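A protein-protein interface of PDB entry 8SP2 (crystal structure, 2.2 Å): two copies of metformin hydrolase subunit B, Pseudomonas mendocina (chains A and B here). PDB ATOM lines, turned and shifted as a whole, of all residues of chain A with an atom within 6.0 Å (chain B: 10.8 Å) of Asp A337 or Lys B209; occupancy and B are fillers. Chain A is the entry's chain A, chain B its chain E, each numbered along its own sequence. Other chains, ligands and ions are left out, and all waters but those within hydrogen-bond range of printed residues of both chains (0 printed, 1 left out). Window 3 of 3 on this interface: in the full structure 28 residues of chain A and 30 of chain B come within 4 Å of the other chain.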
ATOM      1  N   LEU A  10      25.022   7.209 -12.229  1.00  0.00           N
ATOM      2  CA  LEU A  10      24.389   8.183 -11.346  1.00  0.00           C
ATOM      3  C   LEU A  10      25.297   8.551 -10.177  1.00  0.00           C
ATOM      4  O   LEU A  10      25.049   9.556  -9.517  1.00  0.00           O
ATOM      5  CB  LEU A  10      23.085   7.630 -10.759  1.00  0.00           C
ATOM      6  CG  LEU A  10      21.977   7.254 -11.738  1.00  0.00           C
ATOM      7  CD1 LEU A  10      20.735   6.821 -10.977  1.00  0.00           C
ATOM      8  CD2 LEU A  10      21.646   8.405 -12.671  1.00  0.00           C
ATOM      9  N   PHE A  11      26.304   7.722  -9.887  1.00  0.00           N
ATOM     10  CA  PHE A  11      26.968   7.784  -8.592  1.00  0.00           C
ATOM     11  C   PHE A  11      28.473   7.920  -8.775  1.00  0.00           C
ATOM     12  O   PHE A  11      28.997   7.656  -9.860  1.00  0.00           O
ATOM     13  CB  PHE A  11      26.653   6.536  -7.759  1.00  0.00           C
ATOM     14  CG  PHE A  11      25.190   6.299  -7.473  1.00  0.00           C
ATOM     15  CD1 PHE A  11      24.527   7.010  -6.482  1.00  0.00           C
ATOM     16  CD2 PHE A  11      24.480   5.342  -8.184  1.00  0.00           C
ATOM     17  CE1 PHE A  11      23.185   6.779  -6.216  1.00  0.00           C
ATOM     18  CE2 PHE A  11      23.137   5.114  -7.922  1.00  0.00           C
ATOM     19  CZ  PHE A  11      22.489   5.835  -6.940  1.00  0.00           C
ATOM     20  N   SER A  12      29.150   8.319  -7.688  1.00  0.00           N
ATOM     21  CA  SER A  12      30.595   8.446  -7.709  1.00  0.00           C
ATOM     22  C   SER A  12      31.177   7.147  -8.268  1.00  0.00           C
ATOM     23  O   SER A  12      30.702   6.062  -7.933  1.00  0.00           O
ATOM     24  CB  SER A  12      31.151   8.774  -6.339  1.00  0.00           C
ATOM     25  OG  SER A  12      30.317   9.689  -5.638  1.00  0.00           O
ATOM     26  N   TYR A  84      23.745  13.021 -14.576  1.00  0.00           N
ATOM     27  CA  TYR A  84      22.718  13.229 -13.570  1.00  0.00           C
ATOM     28  C   TYR A  84      22.729  14.674 -13.102  1.00  0.00           C
ATOM     29  O   TYR A  84      23.766  15.175 -12.662  1.00  0.00           O
ATOM     30  CB  TYR A  84      22.893  12.311 -12.361  1.00  0.00           C
ATOM     31  CG  TYR A  84      21.861  12.512 -11.279  1.00  0.00           C
ATOM     32  CD1 TYR A  84      20.539  12.142 -11.466  1.00  0.00           C
ATOM     33  CD2 TYR A  84      22.197  13.113 -10.076  1.00  0.00           C
ATOM     34  CE1 TYR A  84      19.586  12.332 -10.475  1.00  0.00           C
ATOM     35  CE2 TYR A  84      21.257  13.320  -9.081  1.00  0.00           C
ATOM     36  CZ  TYR A  84      19.951  12.912  -9.269  1.00  0.00           C
ATOM     37  OH  TYR A  84      19.016  13.102  -8.273  1.00  0.00           O
ATOM     38  N   ASN A  89      16.651  16.210 -10.567  1.00  0.00           N
ATOM     39  CA  ASN A  89      16.473  14.808 -10.241  1.00  0.00           C
ATOM     40  C   ASN A  89      16.274  13.999 -11.520  1.00  0.00           C
ATOM     41  O   ASN A  89      15.464  13.075 -11.552  1.00  0.00           O
ATOM     42  CB  ASN A  89      15.297  14.596  -9.284  1.00  0.00           C
ATOM     43  CG  ASN A  89      15.531  13.479  -8.285  1.00  0.00           C
ATOM     44  OD1 ASN A  89      15.810  12.338  -8.653  1.00  0.00           O
ATOM     45  ND2 ASN A  89      15.429  13.808  -7.006  1.00  0.00           N
ATOM     46  N   ILE A 335      14.210  10.324 -11.428  1.00  0.00           N
ATOM     47  CA  ILE A 335      14.869   9.125 -10.942  1.00  0.00           C
ATOM     48  C   ILE A 335      14.299   8.777  -9.572  1.00  0.00           C
ATOM     49  O   ILE A 335      13.980   9.669  -8.794  1.00  0.00           O
ATOM     50  CB  ILE A 335      16.403   9.309 -10.949  1.00  0.00           C
ATOM     51  CG1 ILE A 335      17.023   8.670 -12.195  1.00  0.00           C
ATOM     52  CG2 ILE A 335      17.059   8.780  -9.683  1.00  0.00           C
ATOM     53  CD1 ILE A 335      16.454   9.177 -13.504  1.00  0.00           C
ATOM     54  N   ASP A 336      14.184   7.466  -9.324  1.00  0.00           N
ATOM     55  CA  ASP A 336      13.688   6.912  -8.076  1.00  0.00           C
ATOM     56  C   ASP A 336      14.528   7.453  -6.926  1.00  0.00           C
ATOM     57  O   ASP A 336      15.725   7.209  -6.863  1.00  0.00           O
ATOM     58  CB  ASP A 336      13.725   5.382  -8.142  1.00  0.00           C
ATOM     59  CG  ASP A 336      13.157   4.637  -6.942  1.00  0.00           C
ATOM     60  OD1 ASP A 336      13.001   5.251  -5.859  1.00  0.00           O
ATOM     61  OD2 ASP A 336      12.889   3.432  -7.099  1.00  0.00           O
ATOM     62  N   ASP A 337      13.877   8.163  -6.003  1.00  0.00           N
ATOM     63  CA  ASP A 337      14.533   8.747  -4.844  1.00  0.00           C
ATOM     64  C   ASP A 337      15.244   7.668  -4.018  1.00  0.00           C
ATOM     65  O   ASP A 337      16.262   7.944  -3.388  1.00  0.00           O
ATOM     66  CB  ASP A 337      13.503   9.508  -4.001  1.00  0.00           C
ATOM     67  CG  ASP A 337      14.007  10.805  -3.388  1.00  0.00           C
ATOM     68  OD1 ASP A 337      15.079  11.279  -3.814  1.00  0.00           O
ATOM     69  OD2 ASP A 337      13.317  11.338  -2.492  1.00  0.00           O
ATOM     70  N   LYS A 338      14.703   6.440  -4.011  1.00  0.00           N
ATOM     71  CA  LYS A 338      15.111   5.409  -3.062  1.00  0.00           C
ATOM     72  C   LYS A 338      16.394   4.706  -3.503  1.00  0.00           C
ATOM     73  O   LYS A 338      17.027   4.021  -2.707  1.00  0.00           O
ATOM     74  CB  LYS A 338      13.979   4.395  -2.871  1.00  0.00           C
ATOM     75  CG  LYS A 338      12.774   4.948  -2.128  1.00  0.00           C
ATOM     76  CD  LYS A 338      11.519   4.144  -2.322  1.00  0.00           C
ATOM     77  CE  LYS A 338      10.453   4.526  -1.319  1.00  0.00           C
ATOM     78  NZ  LYS A 338       9.236   3.697  -1.471  1.00  0.00           N
ATOM     79  N   LEU A 339      16.774   4.892  -4.767  1.00  0.00           N
ATOM     80  CA  LEU A 339      17.991   4.333  -5.334  1.00  0.00           C
ATOM     81  C   LEU A 339      19.211   4.861  -4.577  1.00  0.00           C
ATOM     82  O   LEU A 339      19.292   6.047  -4.285  1.00  0.00           O
ATOM     83  CB  LEU A 339      18.016   4.755  -6.807  1.00  0.00           C
ATOM     84  CG  LEU A 339      18.588   3.764  -7.815  1.00  0.00           C
ATOM     85  CD1 LEU A 339      17.713   2.525  -7.941  1.00  0.00           C
ATOM     86  CD2 LEU A 339      18.721   4.445  -9.164  1.00  0.00           C
ATOM     87  N   ARG A 340      20.158   3.967  -4.261  1.00  0.00           N
ATOM     88  CA  ARG A 340      21.362   4.311  -3.515  1.00  0.00           C
ATOM     89  C   ARG A 340      22.570   3.681  -4.199  1.00  0.00           C
ATOM     90  O   ARG A 340      22.420   2.780  -5.020  1.00  0.00           O
ATOM     91  CB  ARG A 340      21.279   3.810  -2.068  1.00  0.00           C
ATOM     92  CG  ARG A 340      20.247   4.522  -1.205  1.00  0.00           C
ATOM     93  CD  ARG A 340      20.708   5.899  -0.760  1.00  0.00           C
ATOM     94  NE  ARG A 340      19.633   6.646  -0.118  1.00  0.00           N
ATOM     95  CZ  ARG A 340      18.540   7.088  -0.743  1.00  0.00           C
ATOM     96  NH1 ARG A 340      18.428   6.989  -2.058  1.00  0.00           N
ATOM     97  NH2 ARG A 340      17.571   7.669  -0.055  1.00  0.00           N
ATOM     98  N   LEU B 166      29.434  19.916  -4.395  1.00  0.00           N
ATOM     99  CA  LEU B 166      29.286  19.591  -2.982  1.00  0.00           C
ATOM    100  C   LEU B 166      30.513  18.852  -2.460  1.00  0.00           C
ATOM    101  O   LEU B 166      30.946  19.113  -1.335  1.00  0.00           O
ATOM    102  CB  LEU B 166      28.030  18.741  -2.792  1.00  0.00           C
ATOM    103  CG  LEU B 166      26.719  19.470  -3.058  1.00  0.00           C
ATOM    104  CD1 LEU B 166      25.574  18.480  -3.169  1.00  0.00           C
ATOM    105  CD2 LEU B 166      26.452  20.503  -1.969  1.00  0.00           C
ATOM    106  N   ASP B 167      31.058  17.942  -3.289  1.00  0.00           N
ATOM    107  CA  ASP B 167      32.212  17.127  -2.931  1.00  0.00           C
ATOM    108  C   ASP B 167      31.858  16.260  -1.716  1.00  0.00           C
ATOM    109  O   ASP B 167      32.569  16.234  -0.708  1.00  0.00           O
ATOM    110  CB  ASP B 167      33.459  17.985  -2.670  1.00  0.00           C
ATOM    111  CG  ASP B 167      33.863  18.893  -3.819  1.00  0.00           C
ATOM    112  OD1 ASP B 167      33.931  18.383  -4.945  1.00  0.00           O
ATOM    113  OD2 ASP B 167      34.147  20.099  -3.567  1.00  0.00           O
ATOM    114  N   MET B 168      30.749  15.526  -1.835  1.00  0.00           N
ATOM    115  CA  MET B 168      30.249  14.708  -0.746  1.00  0.00           C
ATOM    116  C   MET B 168      30.247  13.234  -1.157  1.00  0.00           C
ATOM    117  O   MET B 168      29.278  12.533  -0.914  1.00  0.00           O
ATOM    118  CB  MET B 168      28.835  15.167  -0.384  1.00  0.00           C
ATOM    119  CG  MET B 168      28.848  16.385   0.502  1.00  0.00           C
ATOM    120  SD  MET B 168      29.234  15.971   2.212  1.00  0.00           S
ATOM    121  CE  MET B 168      27.627  15.369   2.732  1.00  0.00           C
ATOM    122  N   ALA B 169      31.326  12.787  -1.811  1.00  0.00           N
ATOM    123  CA  ALA B 169      31.531  11.378  -2.114  1.00  0.00           C
ATOM    124  C   ALA B 169      32.136  10.690  -0.893  1.00  0.00           C
ATOM    125  O   ALA B 169      33.267  10.988  -0.495  1.00  0.00           O
ATOM    126  CB  ALA B 169      32.426  11.214  -3.324  1.00  0.00           C
ATOM    127  N   ASP B 170      31.358   9.783  -0.298  1.00  0.00           N
ATOM    128  CA  ASP B 170      31.836   9.006   0.830  1.00  0.00           C
ATOM    129  C   ASP B 170      33.144   8.333   0.431  1.00  0.00           C
ATOM    130  O   ASP B 170      34.093   8.355   1.206  1.00  0.00           O
ATOM    131  CB  ASP B 170      30.816   7.976   1.309  1.00  0.00           C
ATOM    132  CG  ASP B 170      31.296   7.284   2.569  1.00  0.00           C
ATOM    133  OD1 ASP B 170      31.611   8.001   3.534  1.00  0.00           O
ATOM    134  OD2 ASP B 170      31.400   6.043   2.558  1.00  0.00           O
ATOM    135  N   SER B 171      33.177   7.779  -0.791  1.00  0.00           N
ATOM    136  CA  SER B 171      34.419   7.366  -1.426  1.00  0.00           C
ATOM    137  C   SER B 171      34.341   7.611  -2.932  1.00  0.00           C
ATOM    138  O   SER B 171      33.263   7.543  -3.520  1.00  0.00           O
ATOM    139  CB  SER B 171      34.734   5.921  -1.143  1.00  0.00           C
ATOM    140  OG  SER B 171      34.037   5.072  -2.041  1.00  0.00           O
ATOM    141  N   TRP B 172      35.513   7.853  -3.535  1.00  0.00           N
ATOM    142  CA  TRP B 172      35.647   8.128  -4.955  1.00  0.00           C
ATOM    143  C   TRP B 172      36.737   7.227  -5.533  1.00  0.00           C
ATOM    144  O   TRP B 172      37.898   7.340  -5.140  1.00  0.00           O
ATOM    145  CB  TRP B 172      35.955   9.621  -5.203  1.00  0.00           C
ATOM    146  CG  TRP B 172      35.932   9.994  -6.656  1.00  0.00           C
ATOM    147  CD1 TRP B 172      36.880   9.717  -7.596  1.00  0.00           C
ATOM    148  CD2 TRP B 172      34.860  10.651  -7.355  1.00  0.00           C
ATOM    149  NE1 TRP B 172      36.486  10.179  -8.823  1.00  0.00           N
ATOM    150  CE2 TRP B 172      35.243  10.744  -8.711  1.00  0.00           C
ATOM    151  CE3 TRP B 172      33.621  11.171  -6.965  1.00  0.00           C
ATOM    152  CZ2 TRP B 172      34.426  11.339  -9.677  1.00  0.00           C
ATOM    153  CZ3 TRP B 172      32.817  11.759  -7.916  1.00  0.00           C
ATOM    154  CH2 TRP B 172      33.220  11.847  -9.252  1.00  0.00           C
ATOM    155  N   PRO B 180      36.722  15.164  -4.583  1.00  0.00           N
ATOM    156  CA  PRO B 180      35.281  14.916  -4.493  1.00  0.00           C
ATOM    157  C   PRO B 180      34.754  14.295  -3.203  1.00  0.00           C
ATOM    158  O   PRO B 180      33.542  14.135  -3.082  1.00  0.00           O
ATOM    159  CB  PRO B 180      34.997  13.876  -5.591  1.00  0.00           C
ATOM    160  CG  PRO B 180      36.178  13.956  -6.535  1.00  0.00           C
ATOM    161  CD  PRO B 180      37.345  14.391  -5.671  1.00  0.00           C
ATOM    162  N   ASN B 204      24.559  22.448 -11.455  1.00  0.00           N
ATOM    163  CA  ASN B 204      24.986  21.726 -12.643  1.00  0.00           C
ATOM    164  C   ASN B 204      25.300  20.273 -12.285  1.00  0.00           C
ATOM    165  O   ASN B 204      24.969  19.820 -11.190  1.00  0.00           O
ATOM    166  CB  ASN B 204      26.107  22.487 -13.350  1.00  0.00           C
ATOM    167  CG  ASN B 204      25.615  23.802 -13.909  1.00  0.00           C
ATOM    168  OD1 ASN B 204      24.428  23.959 -14.186  1.00  0.00           O
ATOM    169  ND2 ASN B 204      26.523  24.739 -14.118  1.00  0.00           N
ATOM    170  N   ALA B 205      25.937  19.546 -13.209  1.00  0.00           N
ATOM    171  CA  ALA B 205      25.837  18.097 -13.229  1.00  0.00           C
ATOM    172  C   ALA B 205      27.025  17.399 -12.569  1.00  0.00           C
ATOM    173  O   ALA B 205      27.039  16.175 -12.560  1.00  0.00           O
ATOM    174  CB  ALA B 205      25.661  17.629 -14.653  1.00  0.00           C
ATOM    175  N   MET B 206      27.981  18.142 -11.984  1.00  0.00           N
ATOM    176  CA  MET B 206      29.137  17.525 -11.340  1.00  0.00           C
ATOM    177  C   MET B 206      28.825  17.242  -9.870  1.00  0.00           C
ATOM    178  O   MET B 206      29.610  17.552  -8.975  1.00  0.00           O
ATOM    179  CB  MET B 206      30.378  18.420 -11.424  1.00  0.00           C
ATOM    180  CG  MET B 206      30.756  18.836 -12.833  1.00  0.00           C
ATOM    181  SD  MET B 206      30.609  17.559 -14.126  1.00  0.00           S
ATOM    182  CE  MET B 206      32.245  17.705 -14.843  1.00  0.00           C
ATOM    183  N   ASN B 207      27.663  16.638  -9.634  1.00  0.00           N
ATOM    184  CA  ASN B 207      27.147  16.402  -8.301  1.00  0.00           C
ATOM    185  C   ASN B 207      26.325  15.119  -8.370  1.00  0.00           C
ATOM    186  O   ASN B 207      25.100  15.154  -8.539  1.00  0.00           O
ATOM    187  CB  ASN B 207      26.324  17.579  -7.772  1.00  0.00           C
ATOM    188  CG  ASN B 207      27.162  18.799  -7.432  1.00  0.00           C
ATOM    189  OD1 ASN B 207      27.891  18.781  -6.443  1.00  0.00           O
ATOM    190  ND2 ASN B 207      27.032  19.867  -8.214  1.00  0.00           N
ATOM    191  N   PRO B 208      26.991  13.945  -8.266  1.00  0.00           N
ATOM    192  CA  PRO B 208      26.306  12.660  -8.366  1.00  0.00           C
ATOM    193  C   PRO B 208      25.337  12.459  -7.201  1.00  0.00           C
ATOM    194  O   PRO B 208      25.473  13.075  -6.138  1.00  0.00           O
ATOM    195  CB  PRO B 208      27.432  11.614  -8.377  1.00  0.00           C
ATOM    196  CG  PRO B 208      28.717  12.410  -8.581  1.00  0.00           C
ATOM    197  CD  PRO B 208      28.433  13.795  -8.046  1.00  0.00           C
ATOM    198  N   LYS B 209      24.358  11.579  -7.439  1.00  0.00           N
ATOM    199  CA  LYS B 209      23.199  11.425  -6.578  1.00  0.00           C
ATOM    200  C   LYS B 209      23.605  11.116  -5.141  1.00  0.00           C
ATOM    201  O   LYS B 209      22.926  11.561  -4.217  1.00  0.00           O
ATOM    202  CB  LYS B 209      22.297  10.308  -7.109  1.00  0.00           C
ATOM    203  CG  LYS B 209      21.006  10.123  -6.327  1.00  0.00           C
ATOM    204  CD  LYS B 209      19.987   9.230  -7.022  1.00  0.00           C
ATOM    205  CE  LYS B 209      18.600   9.366  -6.434  1.00  0.00           C
ATOM    206  NZ  LYS B 209      18.641   9.219  -4.958  1.00  0.00           N
ATOM    207  N   ASP B 210      24.683  10.335  -4.952  1.00  0.00           N
ATOM    208  CA  ASP B 210      25.076   9.933  -3.612  1.00  0.00           C
ATOM    209  C   ASP B 210      25.543  11.145  -2.813  1.00  0.00           C
ATOM    210  O   ASP B 210      25.485  11.111  -1.590  1.00  0.00           O
ATOM    211  CB  ASP B 210      26.140   8.825  -3.577  1.00  0.00           C
ATOM    212  CG  ASP B 210      27.391   9.095  -4.394  1.00  0.00           C
ATOM    213  OD1 ASP B 210      27.251   9.171  -5.630  1.00  0.00           O
ATOM    214  OD2 ASP B 210      28.491   9.218  -3.785  1.00  0.00           O
ATOM    215  N   HIS B 211      26.024  12.198  -3.481  1.00  0.00           N
ATOM    216  CA  HIS B 211      26.451  13.387  -2.761  1.00  0.00           C
ATOM    217  C   HIS B 211      25.227  14.039  -2.121  1.00  0.00           C
ATOM    218  O   HIS B 211      25.311  14.561  -1.009  1.00  0.00           O
ATOM    219  CB  HIS B 211      27.191  14.365  -3.681  1.00  0.00           C
ATOM    220  CG  HIS B 211      28.483  13.869  -4.242  1.00  0.00           C
ATOM    221  ND1 HIS B 211      29.530  14.726  -4.521  1.00  0.00           N
ATOM    222  CD2 HIS B 211      28.882  12.657  -4.637  1.00  0.00           C
ATOM    223  CE1 HIS B 211      30.536  14.038  -5.026  1.00  0.00           C
ATOM    224  NE2 HIS B 211      30.154  12.790  -5.130  1.00  0.00           N
ATOM    225  N   ILE B 212      24.094  14.003  -2.844  1.00  0.00           N
ATOM    226  CA  ILE B 212      22.839  14.558  -2.348  1.00  0.00           C
ATOM    227  C   ILE B 212      22.350  13.681  -1.200  1.00  0.00           C
ATOM    228  O   ILE B 212      22.097  14.198  -0.113  1.00  0.00           O
ATOM    229  CB  ILE B 212      21.766  14.673  -3.453  1.00  0.00           C
ATOM    230  CG1 ILE B 212      22.297  15.387  -4.702  1.00  0.00           C
ATOM    231  CG2 ILE B 212      20.502  15.336  -2.923  1.00  0.00           C
ATOM    232  CD1 ILE B 212      22.993  16.693  -4.421  1.00  0.00           C
ATOM    233  N   ASP B 213      22.235  12.365  -1.479  1.00  0.00           N
ATOM    234  CA  ASP B 213      21.756  11.374  -0.525  1.00  0.00           C
ATOM    235  C   ASP B 213      22.475  11.533   0.816  1.00  0.00           C
ATOM    236  O   ASP B 213      21.832  11.626   1.862  1.00  0.00           O
ATOM    237  CB  ASP B 213      21.948   9.946  -1.054  1.00  0.00           C
ATOM    238  CG  ASP B 213      21.175   9.602  -2.322  1.00  0.00           C
ATOM    239  OD1 ASP B 213      20.062  10.124  -2.500  1.00  0.00           O
ATOM    240  OD2 ASP B 213      21.692   8.796  -3.124  1.00  0.00           O
ATOM    241  N   LEU B 214      23.816  11.554   0.783  1.00  0.00           N
ATOM    242  CA  LEU B 214      24.607  11.659   2.002  1.00  0.00           C
ATOM    243  C   LEU B 214      24.346  12.992   2.701  1.00  0.00           C
ATOM    244  O   LEU B 214      24.270  13.028   3.920  1.00  0.00           O
ATOM    245  CB  LEU B 214      26.098  11.493   1.682  1.00  0.00           C
ATOM    246  CG  LEU B 214      27.000  11.252   2.893  1.00  0.00           C
ATOM    247  CD1 LEU B 214      26.798   9.847   3.449  1.00  0.00           C
ATOM    248  CD2 LEU B 214      28.466  11.478   2.547  1.00  0.00           C
ATOM    249  N   SER B 215      24.231  14.080   1.932  1.00  0.00           N
ATOM    250  CA  SER B 215      24.017  15.401   2.499  1.00  0.00           C
ATOM    251  C   SER B 215      22.721  15.404   3.305  1.00  0.00           C
ATOM    252  O   SER B 215      22.693  15.950   4.407  1.00  0.00           O
ATOM    253  CB  SER B 215      24.008  16.473   1.427  1.00  0.00           C
ATOM    254  OG  SER B 215      25.288  16.608   0.814  1.00  0.00           O
ATOM    255  N   LYS B 216      21.660  14.811   2.731  1.00  0.00           N
ATOM    256  CA  LYS B 216      20.368  14.693   3.398  1.00  0.00           C
ATOM    257  C   LYS B 216      20.526  13.859   4.667  1.00  0.00           C
ATOM    258  O   LYS B 216      20.084  14.280   5.730  1.00  0.00           O
ATOM    259  CB  LYS B 216      19.301  14.008   2.529  1.00  0.00           C
ATOM    260  CG  LYS B 216      18.664  14.831   1.420  1.00  0.00           C
ATOM    261  CD  LYS B 216      17.580  14.054   0.666  1.00  0.00           C
ATOM    262  CE  LYS B 216      17.462  14.408  -0.805  1.00  0.00           C
ATOM    263  NZ  LYS B 216      17.272  15.862  -1.019  1.00  0.00           N
ATOM    264  N   GLU B 217      21.138  12.674   4.525  1.00  0.00           N
ATOM    265  CA  GLU B 217      21.419  11.789   5.648  1.00  0.00           C
ATOM    266  C   GLU B 217      22.057  12.552   6.819  1.00  0.00           C
ATOM    267  O   GLU B 217      21.635  12.391   7.961  1.00  0.00           O
ATOM    268  CB  GLU B 217      22.339  10.631   5.236  1.00  0.00           C
ATOM    269  CG  GLU B 217      21.690   9.254   5.275  1.00  0.00           C
ATOM    270  CD  GLU B 217      22.598   8.148   5.794  1.00  0.00           C
ATOM    271  OE1 GLU B 217      23.839   8.331   5.810  1.00  0.00           O
ATOM    272  OE2 GLU B 217      22.058   7.113   6.225  1.00  0.00           O
ATOM    273  N   TYR B 222      23.163  22.727   2.591  1.00  0.00           N
ATOM    274  CA  TYR B 222      23.834  23.471   1.532  1.00  0.00           C
ATOM    275  C   TYR B 222      22.865  24.444   0.867  1.00  0.00           C
ATOM    276  O   TYR B 222      21.669  24.170   0.773  1.00  0.00           O
ATOM    277  CB  TYR B 222      24.460  22.520   0.506  1.00  0.00           C
ATOM    278  CG  TYR B 222      23.484  21.616  -0.203  1.00  0.00           C
ATOM    279  CD1 TYR B 222      22.754  22.064  -1.292  1.00  0.00           C
ATOM    280  CD2 TYR B 222      23.259  20.325   0.251  1.00  0.00           C
ATOM    281  CE1 TYR B 222      21.861  21.236  -1.947  1.00  0.00           C
ATOM    282  CE2 TYR B 222      22.345  19.493  -0.379  1.00  0.00           C
ATOM    283  CZ  TYR B 222      21.641  19.950  -1.481  1.00  0.00           C
ATOM    284  OH  TYR B 222      20.753  19.123  -2.125  1.00  0.00           O
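The backbone carbonyl oxygen of Asn A89 sits at hydrogen-bond distance from the backbone NH of Ile A335 (3.0 Å).
O of Lys A338 lies within hydrogen-bond range of NH1 of Arg A340 (3.3 Å).
The side-chain amide oxygen (OD1) of Asn B207 lies within hydrogen-bond range of the backbone NH (N) of Leu B166, at 2.8 Å.
N of Met B168 sits at hydrogen-bond distance from ND1 of His B211, at 3.1 Å.
N of Ala B169 lies within hydrogen-bond range of O of Pro B180 (2.9 Å).
O of His B211 lies within hydrogen-bond range of OG of Ser B215 (2.7 Å).
No position is printed for both chains.
Of the 22 pairs that touch across the chains among the printed residues, none has its exchanged pair printed and touching as well.
Of the 23 printed residues of chain B, 10 touch a printed residue of chain A.
Hydrophobic or aromatic side chains of chain B within 4 Å of the printed part of chain A: Ala B169, Trp B172, Ala B205, Pro B208 and His B211.
Among the printed residues, 22 pairs touch across the chains.
Among the printed residues, Asp or Glu carboxylates within 4 Å of a Lys or Arg side-chain nitrogen of the other chain: Arg A340 with Asp B213 (3.6 Å).
Of chain B, only Lys B209 (3.1 Å) comes within 4 Å of Asp A337.
Of chain A, only Leu A10 (3.0 Å), Phe A11 (3.7 Å), Tyr A84 (3.7 Å), Ile A335 (3.6 Å), Asp A336 (3.6 Å), Asp A337 (3.1 Å), Leu A339 (3.3 Å) and Arg A340 (3.7 Å) come within 4 Å of Lys B209.
Asp A336 touches just one residue of chain B: Lys B209.
Of the printed residues of chain A, Ala B205 touches Tyr A84 (3.4 Å).
Printed residues of chain A within 4 Å of Asp B213: Phe A11, Leu A339 and Arg A340.
Printed residues of chain B within 4 Å of Leu A339: Lys B209 (3.3 Å) and Asp B213 (3.8 Å).
Of the printed residues of chain B, Phe A11 touches Pro B208, Lys B209, Asp B210 and Asp B213.
Of the printed residues of chain B, Arg A340 touches Lys B209 and Asp B213.
The backbone carbonyl oxygen (O) of Leu A10 lies within hydrogen-bond range of the backbone NH (N) of Lys B209 (3.0 Å).
OG of Ser A12 is in hydrogen-bond range of OD2 of Asp B210.
OG of Ser A12 is in hydrogen-bond range of NE2 of His B211 (3.1 Å).
O of Asp A337 is in hydrogen-bond range of NZ of Lys B209 (3.1 Å).
The side-chain amino group (NZ) of Lys B209 is in hydrogen-bond range of the backbone carbonyl oxygen (O) of Leu A339, 3.3 Å away.
The side-chain carboxylate (OD1) of Asp B213 lies within salt-bridge range of the guanidinium group (NH1) of Arg A340 (3.6 Å).
O of Tyr A84 sits close to O of Ala B205 (3.4 Å).
Among the printed residues, pairs that only touch across the chains: Leu A10 with Pro B208 (3.3 Å), Phe A11 with Pro B208 (3.9 Å), Phe A11 with Lys B209 (3.7 Å), Phe A11 with Asp B210 (3.3 Å), Phe A11 with Asp B213 (3.98 Å), Ser A12 with Ala B169 (3.5 Å), Ser A12 with Ser B171 (3.7 Å), Ser A12 with Trp B172 (3.5 Å), Ser A12 with Pro B208 (3.8 Å), Tyr A84 with Asn B207 (3.9 Å), Tyr A84 with Lys B209 (3.7 Å), Ile A335 with Lys B209 (3.6 Å), Asp A336 with Lys B209 (3.6 Å), Leu A339 with Asp B213 (3.8 Å) and Arg A340 with Lys B209 (3.7 Å).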
